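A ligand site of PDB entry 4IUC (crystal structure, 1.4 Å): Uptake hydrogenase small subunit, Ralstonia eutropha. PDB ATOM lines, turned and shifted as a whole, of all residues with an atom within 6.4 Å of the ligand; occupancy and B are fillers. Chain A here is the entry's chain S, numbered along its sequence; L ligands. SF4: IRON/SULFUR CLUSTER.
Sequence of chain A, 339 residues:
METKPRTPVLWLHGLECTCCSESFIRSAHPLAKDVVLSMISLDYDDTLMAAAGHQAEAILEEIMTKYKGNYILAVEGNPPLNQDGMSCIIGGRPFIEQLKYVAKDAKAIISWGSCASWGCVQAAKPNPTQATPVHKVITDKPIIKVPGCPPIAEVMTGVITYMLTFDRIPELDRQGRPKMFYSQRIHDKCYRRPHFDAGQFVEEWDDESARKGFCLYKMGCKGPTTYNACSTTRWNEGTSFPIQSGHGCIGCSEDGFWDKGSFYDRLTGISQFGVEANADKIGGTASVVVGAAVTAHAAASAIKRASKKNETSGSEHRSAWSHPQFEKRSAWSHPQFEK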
ATOM      1  N   ILE A 186      21.609   9.744  27.626  1.00  0.00           N
ATOM      2  CA  ILE A 186      21.016   9.474  26.308  1.00  0.00           C
ATOM      3  C   ILE A 186      20.877  10.768  25.486  1.00  0.00           C
ATOM      4  O   ILE A 186      21.181  10.803  24.294  1.00  0.00           O
ATOM      5  CB  ILE A 186      19.610   8.825  26.459  1.00  0.00           C
ATOM      6  CG1 ILE A 186      19.661   7.579  27.339  1.00  0.00           C
ATOM      7  CG2 ILE A 186      19.030   8.471  25.101  1.00  0.00           C
ATOM      8  CD1 ILE A 186      20.551   6.481  26.808  1.00  0.00           C
ATOM      9  N   HIS A 187      20.448  11.825  26.161  1.00  0.00           N
ATOM     10  CA  HIS A 187      20.100  13.108  25.557  1.00  0.00           C
ATOM     11  C   HIS A 187      21.313  13.859  25.008  1.00  0.00           C
ATOM     12  O   HIS A 187      21.167  14.721  24.150  1.00  0.00           O
ATOM     13  CB  HIS A 187      19.363  13.907  26.637  1.00  0.00           C
ATOM     14  CG  HIS A 187      18.836  15.243  26.207  1.00  0.00           C
ATOM     15  ND1 HIS A 187      17.696  15.390  25.465  1.00  0.00           N
ATOM     16  CD2 HIS A 187      19.272  16.527  26.519  1.00  0.00           C
ATOM     17  CE1 HIS A 187      17.466  16.710  25.298  1.00  0.00           C
ATOM     18  NE2 HIS A 187      18.418  17.399  25.938  1.00  0.00           N
ATOM     19  N   ASP A 188      22.515  13.513  25.490  1.00  0.00           N
ATOM     20  CA  ASP A 188      23.744  14.203  25.054  1.00  0.00           C
ATOM     21  C   ASP A 188      23.945  14.090  23.546  1.00  0.00           C
ATOM     22  O   ASP A 188      24.195  15.078  22.859  1.00  0.00           O
ATOM     23  CB  ASP A 188      24.991  13.614  25.760  1.00  0.00           C
ATOM     24  CG  ASP A 188      25.052  13.933  27.259  1.00  0.00           C
ATOM     25  OD1 ASP A 188      24.309  14.808  27.725  1.00  0.00           O
ATOM     26  OD2 ASP A 188      25.899  13.310  27.961  1.00  0.00           O
ATOM     27  N   CYS A 190      21.793  11.973  21.495  1.00  0.00           N
ATOM     28  CA  CYS A 190      20.577  11.530  20.804  1.00  0.00           C
ATOM     29  C   CYS A 190      20.430  12.258  19.466  1.00  0.00           C
ATOM     30  O   CYS A 190      20.505  13.483  19.412  1.00  0.00           O
ATOM     31  CB  CYS A 190      19.354  11.795  21.672  1.00  0.00           C
ATOM     32  SG  CYS A 190      17.794  11.319  20.873  1.00  0.00           S
ATOM     33  N   TYR A 191      20.186  11.500  18.390  1.00  0.00           N
ATOM     34  CA  TYR A 191      20.083  12.094  17.057  1.00  0.00           C
ATOM     35  C   TYR A 191      18.879  13.025  16.921  1.00  0.00           C
ATOM     36  O   TYR A 191      18.815  13.824  15.990  1.00  0.00           O
ATOM     37  CB  TYR A 191      20.083  11.018  15.956  1.00  0.00           C
ATOM     38  CG  TYR A 191      18.738  10.381  15.773  1.00  0.00           C
ATOM     39  CD1 TYR A 191      18.265   9.423  16.689  1.00  0.00           C
ATOM     40  CD2 TYR A 191      17.906  10.744  14.712  1.00  0.00           C
ATOM     41  CE1 TYR A 191      17.010   8.853  16.549  1.00  0.00           C
ATOM     42  CE2 TYR A 191      16.654  10.173  14.559  1.00  0.00           C
ATOM     43  CZ  TYR A 191      16.210   9.231  15.482  1.00  0.00           C
ATOM     44  OH  TYR A 191      14.975   8.682  15.339  1.00  0.00           O
ATOM     45  N   ARG A 192      17.911  12.937  17.848  1.00  0.00           N
ATOM     46  CA  ARG A 192      16.773  13.865  17.823  1.00  0.00           C
ATOM     47  C   ARG A 192      17.043  15.185  18.552  1.00  0.00           C
ATOM     48  O   ARG A 192      16.178  16.064  18.595  1.00  0.00           O
ATOM     49  CB  ARG A 192      15.493  13.203  18.377  1.00  0.00           C
ATOM     50  CG  ARG A 192      15.059  11.977  17.592  1.00  0.00           C
ATOM     51  CD  ARG A 192      13.626  11.562  17.902  1.00  0.00           C
ATOM     52  NE  ARG A 192      13.318  10.312  17.192  1.00  0.00           N
ATOM     53  CZ  ARG A 192      12.091   9.916  16.832  1.00  0.00           C
ATOM     54  NH1 ARG A 192      11.019  10.666  17.102  1.00  0.00           N
ATOM     55  NH2 ARG A 192      11.939   8.778  16.182  1.00  0.00           N
ATOM     56  N   ARG A 193      18.238  15.321  19.117  1.00  0.00           N
ATOM     57  CA  ARG A 193      18.597  16.537  19.876  1.00  0.00           C
ATOM     58  C   ARG A 193      18.412  17.866  19.108  1.00  0.00           C
ATOM     59  O   ARG A 193      17.976  18.851  19.694  1.00  0.00           O
ATOM     60  CB  ARG A 193      20.024  16.412  20.456  1.00  0.00           C
ATOM     61  CG  ARG A 193      20.500  17.591  21.288  1.00  0.00           C
ATOM     62  CD  ARG A 193      19.737  17.720  22.606  1.00  0.00           C
ATOM     63  NE  ARG A 193      20.236  18.835  23.393  1.00  0.00           N
ATOM     64  CZ  ARG A 193      21.251  18.750  24.257  1.00  0.00           C
ATOM     65  NH1 ARG A 193      21.869  17.597  24.460  1.00  0.00           N
ATOM     66  NH2 ARG A 193      21.636  19.832  24.928  1.00  0.00           N
ATOM     67  N   PRO A 194      18.739  17.893  17.783  1.00  0.00           N
ATOM     68  CA  PRO A 194      18.471  19.149  17.068  1.00  0.00           C
ATOM     69  C   PRO A 194      17.009  19.564  17.090  1.00  0.00           C
ATOM     70  O   PRO A 194      16.704  20.751  17.116  1.00  0.00           O
ATOM     71  CB  PRO A 194      18.938  18.847  15.641  1.00  0.00           C
ATOM     72  CG  PRO A 194      20.016  17.842  15.834  1.00  0.00           C
ATOM     73  CD  PRO A 194      19.566  16.967  16.981  1.00  0.00           C
ATOM     74  N   HIS A 195      16.104  18.589  17.090  1.00  0.00           N
ATOM     75  CA  HIS A 195      14.688  18.887  17.233  1.00  0.00           C
ATOM     76  C   HIS A 195      14.346  19.412  18.624  1.00  0.00           C
ATOM     77  O   HIS A 195      13.629  20.411  18.761  1.00  0.00           O
ATOM     78  CB  HIS A 195      13.826  17.668  16.881  1.00  0.00           C
ATOM     79  CG  HIS A 195      13.881  17.303  15.418  1.00  0.00           C
ATOM     80  ND1 HIS A 195      13.602  18.187  14.426  1.00  0.00           N
ATOM     81  CD2 HIS A 195      14.191  16.101  14.788  1.00  0.00           C
ATOM     82  CE1 HIS A 195      13.741  17.581  13.240  1.00  0.00           C
ATOM     83  NE2 HIS A 195      14.092  16.306  13.451  1.00  0.00           N
ATOM     84  N   PHE A 196      14.874  18.763  19.662  1.00  0.00           N
ATOM     85  CA  PHE A 196      14.733  19.258  21.037  1.00  0.00           C
ATOM     86  C   PHE A 196      15.173  20.723  21.145  1.00  0.00           C
ATOM     87  O   PHE A 196      14.451  21.565  21.697  1.00  0.00           O
ATOM     88  CB  PHE A 196      15.541  18.405  22.014  1.00  0.00           C
ATOM     89  CG  PHE A 196      15.502  18.911  23.437  1.00  0.00           C
ATOM     90  CD1 PHE A 196      14.496  18.482  24.312  1.00  0.00           C
ATOM     91  CD2 PHE A 196      16.449  19.837  23.899  1.00  0.00           C
ATOM     92  CE1 PHE A 196      14.442  18.958  25.629  1.00  0.00           C
ATOM     93  CE2 PHE A 196      16.397  20.320  25.209  1.00  0.00           C
ATOM     94  CZ  PHE A 196      15.395  19.877  26.071  1.00  0.00           C
ATOM     95  N   PHE A 201       8.633  18.942  18.742  1.00  0.00           N
ATOM     96  CA  PHE A 201       8.217  17.787  19.542  1.00  0.00           C
ATOM     97  C   PHE A 201       7.048  17.036  18.951  1.00  0.00           C
ATOM     98  O   PHE A 201       6.117  17.637  18.382  1.00  0.00           O
ATOM     99  CB  PHE A 201       7.803  18.239  20.944  1.00  0.00           C
ATOM    100  CG  PHE A 201       8.874  18.996  21.678  1.00  0.00           C
ATOM    101  CD1 PHE A 201       9.968  18.322  22.223  1.00  0.00           C
ATOM    102  CD2 PHE A 201       8.789  20.375  21.832  1.00  0.00           C
ATOM    103  CE1 PHE A 201      10.960  19.020  22.909  1.00  0.00           C
ATOM    104  CE2 PHE A 201       9.778  21.073  22.531  1.00  0.00           C
ATOM    105  CZ  PHE A 201      10.854  20.391  23.064  1.00  0.00           C
ATOM    106  N   PHE A 214      10.563  13.951  15.206  1.00  0.00           N
ATOM    107  CA  PHE A 214      10.719  15.038  16.178  1.00  0.00           C
ATOM    108  C   PHE A 214      10.996  14.485  17.590  1.00  0.00           C
ATOM    109  O   PHE A 214      10.784  13.301  17.858  1.00  0.00           O
ATOM    110  CB  PHE A 214       9.481  15.955  16.180  1.00  0.00           C
ATOM    111  CG  PHE A 214       9.453  16.972  15.074  1.00  0.00           C
ATOM    112  CD1 PHE A 214      10.272  16.848  13.944  1.00  0.00           C
ATOM    113  CD2 PHE A 214       8.594  18.065  15.146  1.00  0.00           C
ATOM    114  CE1 PHE A 214      10.242  17.816  12.933  1.00  0.00           C
ATOM    115  CE2 PHE A 214       8.543  19.012  14.137  1.00  0.00           C
ATOM    116  CZ  PHE A 214       9.377  18.895  13.033  1.00  0.00           C
ATOM    117  N   CYS A 215      11.502  15.347  18.468  1.00  0.00           N
ATOM    118  CA  CYS A 215      11.917  14.932  19.805  1.00  0.00           C
ATOM    119  C   CYS A 215      10.733  14.362  20.586  1.00  0.00           C
ATOM    120  O   CYS A 215       9.574  14.812  20.420  1.00  0.00           O
ATOM    121  CB  CYS A 215      12.575  16.108  20.529  1.00  0.00           C
ATOM    122  SG  CYS A 215      12.816  15.870  22.294  1.00  0.00           S
ATOM    123  N   LEU A 216      11.013  13.356  21.426  1.00  0.00           N
ATOM    124  CA  LEU A 216       9.987  12.620  22.174  1.00  0.00           C
ATOM    125  C   LEU A 216       9.828  13.095  23.625  1.00  0.00           C
ATOM    126  O   LEU A 216       9.128  12.475  24.417  1.00  0.00           O
ATOM    127  CB  LEU A 216      10.304  11.122  22.138  1.00  0.00           C
ATOM    128  CG  LEU A 216      10.197  10.499  20.738  1.00  0.00           C
ATOM    129  CD1 LEU A 216      10.905   9.147  20.688  1.00  0.00           C
ATOM    130  CD2 LEU A 216       8.746  10.363  20.292  1.00  0.00           C
ATOM    131  N   TYR A 217      10.440  14.243  23.952  1.00  0.00           N
ATOM    132  CA  TYR A 217      10.381  14.776  25.326  1.00  0.00           C
ATOM    133  C   TYR A 217       8.958  14.902  25.854  1.00  0.00           C
ATOM    134  O   TYR A 217       8.678  14.527  26.996  1.00  0.00           O
ATOM    135  CB  TYR A 217      11.088  16.135  25.369  1.00  0.00           C
ATOM    136  CG  TYR A 217      11.201  16.758  26.741  1.00  0.00           C
ATOM    137  CD1 TYR A 217      12.309  16.499  27.549  1.00  0.00           C
ATOM    138  CD2 TYR A 217      10.228  17.627  27.223  1.00  0.00           C
ATOM    139  CE1 TYR A 217      12.454  17.079  28.798  1.00  0.00           C
ATOM    140  CE2 TYR A 217      10.350  18.220  28.481  1.00  0.00           C
ATOM    141  CZ  TYR A 217      11.463  17.939  29.268  1.00  0.00           C
ATOM    142  OH  TYR A 217      11.604  18.540  30.494  1.00  0.00           O
ATOM    143  N   LYS A 218       8.061  15.430  25.032  1.00  0.00           N
ATOM    144  CA  LYS A 218       6.678  15.655  25.467  1.00  0.00           C
ATOM    145  C   LYS A 218       5.845  14.378  25.509  1.00  0.00           C
ATOM    146  O   LYS A 218       4.723  14.380  26.047  1.00  0.00           O
ATOM    147  CB  LYS A 218       6.003  16.748  24.631  1.00  0.00           C
ATOM    148  CG  LYS A 218       6.699  18.095  24.802  1.00  0.00           C
ATOM    149  CD  LYS A 218       5.991  19.209  24.052  1.00  0.00           C
ATOM    150  CE  LYS A 218       6.533  20.569  24.506  1.00  0.00           C
ATOM    151  NZ  LYS A 218       5.946  21.701  23.728  1.00  0.00           N
ATOM    152  N   CYS A 221       9.867  11.042  27.166  1.00  0.00           N
ATOM    153  CA  CYS A 221      11.240  10.559  27.057  1.00  0.00           C
ATOM    154  C   CYS A 221      12.081  10.955  28.268  1.00  0.00           C
ATOM    155  O   CYS A 221      12.178  12.136  28.591  1.00  0.00           O
ATOM    156  CB  CYS A 221      11.895  11.078  25.796  1.00  0.00           C
ATOM    157  SG  CYS A 221      13.573  10.433  25.559  1.00  0.00           S
ATOM    158  N   LYS A 222      12.712   9.964  28.896  1.00  0.00           N
ATOM    159  CA  LYS A 222      13.555  10.189  30.080  1.00  0.00           C
ATOM    160  C   LYS A 222      15.035  10.215  29.718  1.00  0.00           C
ATOM    161  O   LYS A 222      15.920  10.169  30.607  1.00  0.00           O
ATOM    162  CB  LYS A 222      13.255   9.169  31.185  1.00  0.00           C
ATOM    163  CG  LYS A 222      11.784   9.166  31.629  1.00  0.00           C
ATOM    164  CD  LYS A 222      11.329  10.593  31.981  1.00  0.00           C
ATOM    165  CE  LYS A 222       9.968  10.653  32.686  1.00  0.00           C
ATOM    166  NZ  LYS A 222       8.855   9.993  31.941  1.00  0.00           N
ATOM    167  N   GLY A 223      15.332  10.334  28.421  1.00  0.00           N
ATOM    168  CA  GLY A 223      16.718  10.483  27.962  1.00  0.00           C
ATOM    169  C   GLY A 223      17.534  11.565  28.682  1.00  0.00           C
ATOM    170  O   GLY A 223      18.724  11.357  28.942  1.00  0.00           O
ATOM    171  N   PRO A 224      16.911  12.725  29.002  1.00  0.00           N
ATOM    172  CA  PRO A 224      17.689  13.791  29.669  1.00  0.00           C
ATOM    173  C   PRO A 224      18.232  13.458  31.059  1.00  0.00           C
ATOM    174  O   PRO A 224      19.145  14.129  31.528  1.00  0.00           O
ATOM    175  CB  PRO A 224      16.680  14.942  29.755  1.00  0.00           C
ATOM    176  CG  PRO A 224      15.807  14.730  28.564  1.00  0.00           C
ATOM    177  CD  PRO A 224      15.615  13.245  28.503  1.00  0.00           C
ATOM    178  N   SER A 231      22.353   5.879  22.690  1.00  0.00           N
ATOM    179  CA  SER A 231      22.306   6.853  21.580  1.00  0.00           C
ATOM    180  C   SER A 231      23.451   6.691  20.597  1.00  0.00           C
ATOM    181  O   SER A 231      23.369   7.140  19.452  1.00  0.00           O
ATOM    182  CB  SER A 231      22.321   8.276  22.114  1.00  0.00           C
ATOM    183  OG  SER A 231      21.148   8.554  22.820  1.00  0.00           O
ATOM    184  N   PHE A 241      17.682   2.030  18.555  1.00  0.00           N
ATOM    185  CA  PHE A 241      17.505   2.151  20.004  1.00  0.00           C
ATOM    186  C   PHE A 241      16.091   2.663  20.234  1.00  0.00           C
ATOM    187  O   PHE A 241      15.429   3.061  19.273  1.00  0.00           O
ATOM    188  CB  PHE A 241      18.634   2.987  20.701  1.00  0.00           C
ATOM    189  CG  PHE A 241      18.581   4.482  20.461  1.00  0.00           C
ATOM    190  CD1 PHE A 241      18.786   5.023  19.182  1.00  0.00           C
ATOM    191  CD2 PHE A 241      18.440   5.362  21.535  1.00  0.00           C
ATOM    192  CE1 PHE A 241      18.808   6.408  18.990  1.00  0.00           C
ATOM    193  CE2 PHE A 241      18.471   6.747  21.345  1.00  0.00           C
ATOM    194  CZ  PHE A 241      18.646   7.266  20.067  1.00  0.00           C
ATOM    195  N   ILE A 243      14.508   5.314  21.064  1.00  0.00           N
ATOM    196  CA  ILE A 243      14.124   6.596  20.481  1.00  0.00           C
ATOM    197  C   ILE A 243      14.113   6.547  18.949  1.00  0.00           C
ATOM    198  O   ILE A 243      13.192   7.062  18.309  1.00  0.00           O
ATOM    199  CB  ILE A 243      15.047   7.714  21.016  1.00  0.00           C
ATOM    200  CG1 ILE A 243      14.666   8.026  22.471  1.00  0.00           C
ATOM    201  CG2 ILE A 243      14.993   8.967  20.143  1.00  0.00           C
ATOM    202  CD1 ILE A 243      15.837   8.420  23.349  1.00  0.00           C
ATOM    203  N   GLY A 248       9.902   7.033  23.571  1.00  0.00           N
ATOM    204  CA  GLY A 248      10.847   7.668  24.500  1.00  0.00           C
ATOM    205  C   GLY A 248      11.597   6.663  25.355  1.00  0.00           C
ATOM    206  O   GLY A 248      11.126   5.555  25.616  1.00  0.00           O
ATOM    207  N   CYS A 249      12.795   7.044  25.751  1.00  0.00           N
ATOM    208  CA  CYS A 249      13.497   6.316  26.803  1.00  0.00           C
ATOM    209  C   CYS A 249      12.593   6.284  28.044  1.00  0.00           C
ATOM    210  O   CYS A 249      11.933   7.287  28.370  1.00  0.00           O
ATOM    211  CB  CYS A 249      14.824   7.046  27.091  1.00  0.00           C
ATOM    212  SG  CYS A 249      15.816   6.423  28.455  1.00  0.00           S
HETATM  213 FE1  SF4 L   1      16.475  14.101  24.450  1.00  0.00          FE
HETATM  214 FE2  SF4 L   1      14.602  12.082  24.340  1.00  0.00          FE
HETATM  215 FE3  SF4 L   1      16.373  12.434  22.300  1.00  0.00          FE
HETATM  216 FE4  SF4 L   1      14.394  14.261  22.717  1.00  0.00          FE
HETATM  217  S1  SF4 L   1      14.164  12.152  22.104  1.00  0.00           S
HETATM  218  S2  SF4 L   1      16.561  14.703  22.231  1.00  0.00           S
HETATM  219  S3  SF4 L   1      14.261  14.175  25.015  1.00  0.00           S
HETATM  220  S4  SF4 L   1      16.866  11.898  24.465  1.00  0.00           S
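FE1 of the ligand is bound by ND1 of His 187, at 2.0 Å.
An iron atom (FE4) of the ligand is bound by the side-chain sulfur (SG) of Cys 215.
An iron atom (FE2) of the ligand is bound by the side-chain sulfur (SG) of Cys 221, 2.3 Å away.
SG of Cys 190 binds FE3 of the ligand, at 2.3 Å.
A sulfur (S1) of the ligand lies close to the backbone NH (N) of Leu 216 (3.4 Å).
The backbone NH (N) of Arg 193 sits close to a sulfur (S2) of the ligand, 3.6 Å away.
The backbone carbonyl oxygen of His 187 is in hydrogen-bond range of the guanidinium group of Arg 193, 3.0 Å away.
The backbone carbonyl oxygen (O) of Gly 223 is in hydrogen-bond range of the backbone NH (N) of His 187.
The side-chain sulfur (SG) of Cys 215 lies close to the backbone NH (N) of Tyr 217, 3.3 Å away.
The backbone NH (N) of Gly 223 sits close to the side-chain sulfur (SG) of Cys 221 (3.4 Å).
The side-chain sulfur of Cys 190 sits close to the backbone NH of Arg 192 (3.4 Å).
NH2 of Arg 192 lies within hydrogen-bond range of O of Ile 243 (3.0 Å).
The guanidinium group of Arg 192 is in hydrogen-bond range of the side-chain hydroxyl of Tyr 191, at 3.0 Å.
The guanidinium group (NH1) of Arg 192 lies within hydrogen-bond range of the backbone carbonyl oxygen (O) of Phe 214 (2.8 Å).
C of Arg 192 touches S2 of the ligand (3.7 Å).
CB of Phe 196 touches S2 of the ligand (3.8 Å).
Tyr 217 touches the ligand (CB to S3, 3.7 Å).
Gly 223 touches the ligand.
CD of Pro 224 touches S3 of the ligand, at 3.9 Å.
Ile 243 touches the ligand (CD1 to S4, 3.8 Å).
Hydrophobic or aromatic side chains within 4 Å of the ligand: His 187, Phe 196, Leu 216, Tyr 217, Pro 224 and Ile 243.
12 residues have an atom within 4 Å of the ligand: His 187, Cys 190, Arg 192, Arg 193, Phe 196, Cys 215, Leu 216, Tyr 217, Cys 221, Gly 223, Pro 224 and Ile 243.
The nearest printed residue that does not touch the ligand is Ile 186 (4.1 Å).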
